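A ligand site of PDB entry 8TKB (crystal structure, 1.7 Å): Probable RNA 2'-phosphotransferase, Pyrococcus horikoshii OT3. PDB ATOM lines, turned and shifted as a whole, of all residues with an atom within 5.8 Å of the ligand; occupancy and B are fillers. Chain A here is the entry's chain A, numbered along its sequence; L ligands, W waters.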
ATOM      1  N   HIS A  95     -28.070   3.607 -19.868  1.00  0.00           N
ATOM      2  CA  HIS A  95     -27.991   4.203 -21.207  1.00  0.00           C
ATOM      3  C   HIS A  95     -28.283   5.692 -21.084  1.00  0.00           C
ATOM      4  O   HIS A  95     -29.438   6.061 -20.806  1.00  0.00           O
ATOM      5  CB  HIS A  95     -29.003   3.563 -22.160  1.00  0.00           C
ATOM      6  CG  HIS A  95     -29.010   4.167 -23.539  1.00  0.00           C
ATOM      7  ND1 HIS A  95     -28.028   3.911 -24.469  1.00  0.00           N
ATOM      8  CD2 HIS A  95     -29.893   5.024 -24.143  1.00  0.00           C
ATOM      9  CE1 HIS A  95     -28.290   4.577 -25.581  1.00  0.00           C
ATOM     10  NE2 HIS A  95     -29.402   5.269 -25.413  1.00  0.00           N
ATOM     11  N   GLY A  96     -27.293   6.536 -21.356  1.00  0.00           N
ATOM     12  CA  GLY A  96     -27.497   7.968 -21.343  1.00  0.00           C
ATOM     13  C   GLY A  96     -27.994   8.467 -22.682  1.00  0.00           C
ATOM     14  O   GLY A  96     -27.420   8.138 -23.731  1.00  0.00           O
ATOM     15  N   THR A  97     -29.060   9.271 -22.654  1.00  0.00           N
ATOM     16  CA  THR A  97     -29.592   9.801 -23.915  1.00  0.00           C
ATOM     17  C   THR A  97     -30.264  11.131 -23.596  1.00  0.00           C
ATOM     18  O   THR A  97     -29.984  11.717 -22.547  1.00  0.00           O
ATOM     19  CB  THR A  97     -30.499   8.770 -24.601  1.00  0.00           C
ATOM     20  OG1 THR A  97     -30.851   9.239 -25.908  1.00  0.00           O
ATOM     21  CG2 THR A  97     -31.750   8.446 -23.771  1.00  0.00           C
ATOM     22  N   VAL A  98     -31.112  11.613 -24.493  1.00  0.00           N
ATOM     23  CA  VAL A  98     -31.809  12.882 -24.279  1.00  0.00           C
ATOM     24  C   VAL A  98     -33.319  12.624 -24.274  1.00  0.00           C
ATOM     25  O   VAL A  98     -33.832  11.679 -24.881  1.00  0.00           O
ATOM     26  CB  VAL A  98     -31.451  13.958 -25.324  1.00  0.00           C
ATOM     27  CG1 VAL A  98     -30.041  14.533 -25.041  1.00  0.00           C
ATOM     28  CG2 VAL A  98     -31.574  13.424 -26.757  1.00  0.00           C
ATOM     29  N   ASN A 101     -35.769  11.632 -27.151  1.00  0.00           N
ATOM     30  CA  ASN A 101     -35.789  10.259 -27.660  1.00  0.00           C
ATOM     31  C   ASN A 101     -36.710   9.338 -26.866  1.00  0.00           C
ATOM     32  O   ASN A 101     -36.919   8.199 -27.279  1.00  0.00           O
ATOM     33  CB  ASN A 101     -34.384   9.660 -27.646  1.00  0.00           C
ATOM     34  CG  ASN A 101     -33.458  10.298 -28.648  1.00  0.00           C
ATOM     35  OD1 ASN A 101     -33.902  10.910 -29.611  1.00  0.00           O
ATOM     36  ND2 ASN A 101     -32.120  10.189 -28.406  1.00  0.00           N
ATOM     37  N   GLY A 104     -39.836   7.728 -28.796  1.00  0.00           N
ATOM     38  CA  GLY A 104     -39.444   6.649 -29.678  1.00  0.00           C
ATOM     39  C   GLY A 104     -38.924   5.445 -28.920  1.00  0.00           C
ATOM     40  O   GLY A 104     -39.210   4.297 -29.284  1.00  0.00           O
ATOM     41  N   ILE A 105     -38.143   5.692 -27.861  1.00  0.00           N
ATOM     42  CA  ILE A 105     -37.582   4.569 -27.137  1.00  0.00           C
ATOM     43  C   ILE A 105     -38.674   3.829 -26.386  1.00  0.00           C
ATOM     44  O   ILE A 105     -38.624   2.600 -26.276  1.00  0.00           O
ATOM     45  CB  ILE A 105     -36.472   5.069 -26.190  1.00  0.00           C
ATOM     46  CG1 ILE A 105     -35.267   5.508 -27.045  1.00  0.00           C
ATOM     47  CG2 ILE A 105     -36.056   3.980 -25.202  1.00  0.00           C
ATOM     48  CD1 ILE A 105     -34.186   6.202 -26.214  1.00  0.00           C
ATOM     49  N   GLU A 108     -40.358   1.646 -29.193  1.00  0.00           N
ATOM     50  CA  GLU A 108     -39.529   0.816 -30.060  1.00  0.00           C
ATOM     51  C   GLU A 108     -38.370   0.132 -29.327  1.00  0.00           C
ATOM     52  O   GLU A 108     -37.740  -0.762 -29.902  1.00  0.00           O
ATOM     53  CB  GLU A 108     -38.941   1.714 -31.157  1.00  0.00           C
ATOM     54  CG  GLU A 108     -39.746   1.816 -32.433  1.00  0.00           C
ATOM     55  CD  GLU A 108     -39.083   2.764 -33.433  1.00  0.00           C
ATOM     56  OE1 GLU A 108     -38.273   2.290 -34.261  1.00  0.00           O
ATOM     57  OE2 GLU A 108     -39.337   3.978 -33.343  1.00  0.00           O
ATOM     58  N   GLY A 109     -38.079   0.525 -28.090  1.00  0.00           N
ATOM     59  CA  GLY A 109     -36.871   0.066 -27.421  1.00  0.00           C
ATOM     60  C   GLY A 109     -35.690   0.908 -27.868  1.00  0.00           C
ATOM     61  O   GLY A 109     -35.797   1.814 -28.699  1.00  0.00           O
ATOM     62  N   ILE A 110     -34.517   0.592 -27.319  1.00  0.00           N
ATOM     63  CA  ILE A 110     -33.297   1.269 -27.714  1.00  0.00           C
ATOM     64  C   ILE A 110     -32.737   0.536 -28.914  1.00  0.00           C
ATOM     65  O   ILE A 110     -32.357  -0.638 -28.817  1.00  0.00           O
ATOM     66  CB  ILE A 110     -32.271   1.319 -26.574  1.00  0.00           C
ATOM     67  CG1 ILE A 110     -32.935   1.724 -25.274  1.00  0.00           C
ATOM     68  CG2 ILE A 110     -31.077   2.259 -26.969  1.00  0.00           C
ATOM     69  CD1 ILE A 110     -31.889   1.677 -24.128  1.00  0.00           C
ATOM     70  N   LYS A 111     -32.719   1.220 -30.077  1.00  0.00           N
ATOM     71  CA  LYS A 111     -32.436   0.630 -31.377  1.00  0.00           C
ATOM     72  C   LYS A 111     -31.101   1.126 -31.893  1.00  0.00           C
ATOM     73  O   LYS A 111     -30.699   2.255 -31.594  1.00  0.00           O
ATOM     74  CB  LYS A 111     -33.489   1.018 -32.435  1.00  0.00           C
ATOM     75  CG  LYS A 111     -34.826   0.389 -32.315  1.00  0.00           C
ATOM     76  CD  LYS A 111     -35.744   1.034 -33.353  1.00  0.00           C
ATOM     77  CE  LYS A 111     -34.967   1.577 -34.561  1.00  0.00           C
ATOM     78  NZ  LYS A 111     -35.445   2.925 -35.008  1.00  0.00           N
ATOM     79  N   PRO A 112     -30.390   0.311 -32.677  1.00  0.00           N
ATOM     80  CA  PRO A 112     -29.231   0.831 -33.409  1.00  0.00           C
ATOM     81  C   PRO A 112     -29.712   1.889 -34.383  1.00  0.00           C
ATOM     82  O   PRO A 112     -30.771   1.749 -35.007  1.00  0.00           O
ATOM     83  CB  PRO A 112     -28.668  -0.397 -34.144  1.00  0.00           C
ATOM     84  CG  PRO A 112     -29.593  -1.524 -33.883  1.00  0.00           C
ATOM     85  CD  PRO A 112     -30.620  -1.128 -32.886  1.00  0.00           C
ATOM     86  N   MET A 113     -28.959   2.977 -34.479  1.00  0.00           N
ATOM     87  CA  MET A 113     -29.414   4.147 -35.206  1.00  0.00           C
ATOM     88  C   MET A 113     -28.552   4.407 -36.433  1.00  0.00           C
ATOM     89  O   MET A 113     -29.045   4.437 -37.572  1.00  0.00           O
ATOM     90  CB  MET A 113     -29.429   5.346 -34.249  1.00  0.00           C
ATOM     91  CG  MET A 113     -29.841   6.651 -34.879  1.00  0.00           C
ATOM     92  SD  MET A 113     -31.638   6.697 -35.128  1.00  0.00           S
ATOM     93  CE  MET A 113     -32.275   5.618 -33.837  1.00  0.00           C
ATOM     94  N   LYS A 114     -27.252   4.587 -36.237  1.00  0.00           N
ATOM     95  CA  LYS A 114     -26.338   4.542 -37.367  1.00  0.00           C
ATOM     96  C   LYS A 114     -25.347   3.408 -37.187  1.00  0.00           C
ATOM     97  O   LYS A 114     -25.125   2.612 -38.104  1.00  0.00           O
ATOM     98  CB  LYS A 114     -25.594   5.874 -37.539  1.00  0.00           C
ATOM     99  CG  LYS A 114     -24.243   5.758 -38.285  1.00  0.00           C
ATOM    100  CD  LYS A 114     -23.627   7.152 -38.425  1.00  0.00           C
ATOM    101  CE  LYS A 114     -22.539   7.251 -39.447  1.00  0.00           C
ATOM    102  NZ  LYS A 114     -21.347   6.397 -39.095  1.00  0.00           N
ATOM    103  N   ARG A 115     -24.742   3.326 -36.005  1.00  0.00           N
ATOM    104  CA  ARG A 115     -23.916   2.177 -35.705  1.00  0.00           C
ATOM    105  C   ARG A 115     -24.806   0.973 -35.472  1.00  0.00           C
ATOM    106  O   ARG A 115     -26.007   1.099 -35.177  1.00  0.00           O
ATOM    107  CB  ARG A 115     -23.047   2.474 -34.482  1.00  0.00           C
ATOM    108  CG  ARG A 115     -21.834   3.353 -34.819  1.00  0.00           C
ATOM    109  CD  ARG A 115     -22.116   4.881 -34.757  1.00  0.00           C
ATOM    110  NE  ARG A 115     -22.171   5.383 -33.389  1.00  0.00           N
ATOM    111  CZ  ARG A 115     -21.127   5.851 -32.702  1.00  0.00           C
ATOM    112  NH1 ARG A 115     -19.912   5.913 -33.245  1.00  0.00           N
ATOM    113  NH2 ARG A 115     -21.292   6.246 -31.443  1.00  0.00           N
ATOM    114  N   TYR A 117     -24.645  -1.283 -33.158  1.00  0.00           N
ATOM    115  CA  TYR A 117     -24.643  -1.705 -31.758  1.00  0.00           C
ATOM    116  C   TYR A 117     -25.255  -0.617 -30.892  1.00  0.00           C
ATOM    117  O   TYR A 117     -24.973   0.556 -31.131  1.00  0.00           O
ATOM    118  CB  TYR A 117     -23.181  -1.953 -31.287  1.00  0.00           C
ATOM    119  CG  TYR A 117     -22.422  -2.953 -32.129  1.00  0.00           C
ATOM    120  CD1 TYR A 117     -22.514  -4.309 -31.844  1.00  0.00           C
ATOM    121  CD2 TYR A 117     -21.604  -2.544 -33.181  1.00  0.00           C
ATOM    122  CE1 TYR A 117     -21.827  -5.243 -32.612  1.00  0.00           C
ATOM    123  CE2 TYR A 117     -20.908  -3.481 -33.939  1.00  0.00           C
ATOM    124  CZ  TYR A 117     -21.021  -4.838 -33.646  1.00  0.00           C
ATOM    125  OH  TYR A 117     -20.337  -5.787 -34.399  1.00  0.00           O
ATOM    126  N   VAL A 118     -26.068  -0.999 -29.863  1.00  0.00           N
ATOM    127  CA  VAL A 118     -26.521  -0.068 -28.822  1.00  0.00           C
ATOM    128  C   VAL A 118     -25.420   0.035 -27.772  1.00  0.00           C
ATOM    129  O   VAL A 118     -24.846  -0.984 -27.362  1.00  0.00           O
ATOM    130  CB  VAL A 118     -27.838  -0.550 -28.184  1.00  0.00           C
ATOM    131  CG1 VAL A 118     -28.185   0.320 -26.968  1.00  0.00           C
ATOM    132  CG2 VAL A 118     -28.951  -0.560 -29.229  1.00  0.00           C
ATOM    133  N   HIS A 119     -25.137   1.266 -27.301  1.00  0.00           N
ATOM    134  CA  HIS A 119     -24.090   1.485 -26.308  1.00  0.00           C
ATOM    135  C   HIS A 119     -24.705   1.652 -24.924  1.00  0.00           C
ATOM    136  O   HIS A 119     -25.594   2.479 -24.729  1.00  0.00           O
ATOM    137  CB  HIS A 119     -23.248   2.710 -26.636  1.00  0.00           C
ATOM    138  CG  HIS A 119     -22.462   2.566 -27.896  1.00  0.00           C
ATOM    139  ND1 HIS A 119     -22.901   3.066 -29.111  1.00  0.00           N
ATOM    140  CD2 HIS A 119     -21.284   1.938 -28.152  1.00  0.00           C
ATOM    141  CE1 HIS A 119     -22.033   2.767 -30.048  1.00  0.00           C
ATOM    142  NE2 HIS A 119     -21.035   2.088 -29.503  1.00  0.00           N
ATOM    143  N   HIS A 134     -25.252  14.744 -26.373  1.00  0.00           N
ATOM    144  CA  HIS A 134     -26.350  15.029 -27.288  1.00  0.00           C
ATOM    145  C   HIS A 134     -27.227  16.164 -26.833  1.00  0.00           C
ATOM    146  O   HIS A 134     -28.203  16.497 -27.518  1.00  0.00           O
ATOM    147  CB  HIS A 134     -27.176  13.780 -27.512  1.00  0.00           C
ATOM    148  CG  HIS A 134     -26.427  12.748 -28.280  1.00  0.00           C
ATOM    149  ND1 HIS A 134     -26.350  12.771 -29.660  1.00  0.00           N
ATOM    150  CD2 HIS A 134     -25.674  11.698 -27.876  1.00  0.00           C
ATOM    151  CE1 HIS A 134     -25.597  11.765 -30.063  1.00  0.00           C
ATOM    152  NE2 HIS A 134     -25.189  11.086 -29.009  1.00  0.00           N
HETATM  153  P1  LIG L   1     -24.819   6.071 -30.645  1.00  0.00           P
HETATM  154  O1  LIG L   1     -25.174   4.666 -30.210  1.00  0.00           O
HETATM  155  O2  LIG L   1     -23.744   6.820 -29.893  1.00  0.00           O
HETATM  156  O3  LIG L   1     -24.637   6.181 -32.164  1.00  0.00           O
HETATM  157  O4  LIG L   1     -26.142   6.915 -30.345  1.00  0.00           O
HETATM  158  C1  LIG L   1     -27.407   6.482 -30.820  1.00  0.00           C
HETATM  159  C2  LIG L   1     -28.518   7.379 -30.287  1.00  0.00           C
HETATM  160  O5  LIG L   1     -29.822   6.897 -30.729  1.00  0.00           O
HETATM  161  C3  LIG L   1     -28.583   7.451 -28.741  1.00  0.00           C
HETATM  162  O6  LIG L   1     -28.777   8.815 -28.327  1.00  0.00           O
HETATM  163  C4  LIG L   1     -29.821   6.619 -28.415  1.00  0.00           C
HETATM  164  O7  LIG L   1     -30.438   6.923 -27.170  1.00  0.00           O
HETATM  165  C5  LIG L   1     -30.712   6.938 -29.629  1.00  0.00           C
HETATM  166  N1  LIG L   1     -31.821   6.000 -29.852  1.00  0.00           N
HETATM  167  C6  LIG L   1     -31.784   4.636 -29.741  1.00  0.00           C
HETATM  168  N2  LIG L   1     -32.936   4.062 -29.980  1.00  0.00           N
HETATM  169  C7  LIG L   1     -33.806   5.108 -30.243  1.00  0.00           C
HETATM  170  C8  LIG L   1     -35.176   5.133 -30.546  1.00  0.00           C
HETATM  171  N3  LIG L   1     -35.948   4.044 -30.652  1.00  0.00           N
HETATM  172  N4  LIG L   1     -35.743   6.351 -30.749  1.00  0.00           N
HETATM  173  C9  LIG L   1     -34.971   7.440 -30.642  1.00  0.00           C
HETATM  174  N5  LIG L   1     -33.670   7.527 -30.348  1.00  0.00           N
HETATM  175  C10 LIG L   1     -33.133   6.312 -30.147  1.00  0.00           C
HETATM  176  O   HOH W   1     -26.296   2.730 -31.703  1.00  0.00           O
HETATM  177  O   HOH W   2     -26.146   4.497 -33.783  1.00  0.00           O
HETATM  178  O   HOH W   3     -27.113   8.790 -26.314  1.00  0.00           O
HETATM  179  O   HOH W   4     -29.435  10.916 -29.808  1.00  0.00           O
HETATM  180  O   HOH W   5     -31.495   9.642 -32.043  1.00  0.00           O
HETATM  181  O   HOH W   6     -37.594   6.746 -32.942  1.00  0.00           O
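The side-chain hydroxyl (OG1) of Thr 97 is in hydrogen-bond range of an oxygen (O7) of the ligand (2.7 Å).
N5 of the ligand lies close to OD1 of Asn 101 (3.5 Å).
NE of Arg 115 lies within salt-bridge range of O3 of the ligand, at 2.9 Å.
A ring nitrogen (ND1) of His 119 lies within hydrogen-bond range of an oxygen (O1) of the ligand.
O of Gly 109 lies within hydrogen-bond range of N3 of the ligand, 3.0 Å away.
The backbone NH (N) of Lys 111 sits at hydrogen-bond distance from a nitrogen (N2) of the ligand, 2.9 Å away.
A ring nitrogen (NE2) of His 95 sits at hydrogen-bond distance from an oxygen (O7) of the ligand (2.6 Å).
OE1 of Glu 108 is in salt-bridge range of NZ of Lys 111 (3.0 Å).
The side-chain amide nitrogen (ND2) of Asn 101 sits at hydrogen-bond distance from the side-chain hydroxyl (OG1) of Thr 97.
O of His 119 lies within hydrogen-bond range of ND1 of His 95, at 2.8 Å.
Merely in contact with the ligand: Ile 105, Gly 104, Ile 110, Glu 108 and Met 113.
Within 4 Å of the ligand: His 95, Thr 97, Asn 101, Gly 104, Ile 105, Glu 108, Gly 109, Ile 110, Lys 111, Met 113, Arg 115 and His 119.
Along chain A the residues within 4 Å of the ligand span positions 95 to 119.
Water W3 bridges O6 of the ligand and O of Gly 96.
Water W4 lies within hydrogen-bond range of an oxygen (O6) of the ligand (2.7 Å) and the side-chain amide nitrogen of Asn 101 (3.1 Å).
Water W1 bridges the backbone carbonyl oxygen of Tyr 117 (2.6 Å) and an oxygen (O1) of the ligand (2.7 Å).
Water W6 lies within hydrogen-bond range of a nitrogen (N4) of the ligand (2.9 Å) and the side-chain carboxylate of Glu 108 (3.3 Å).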
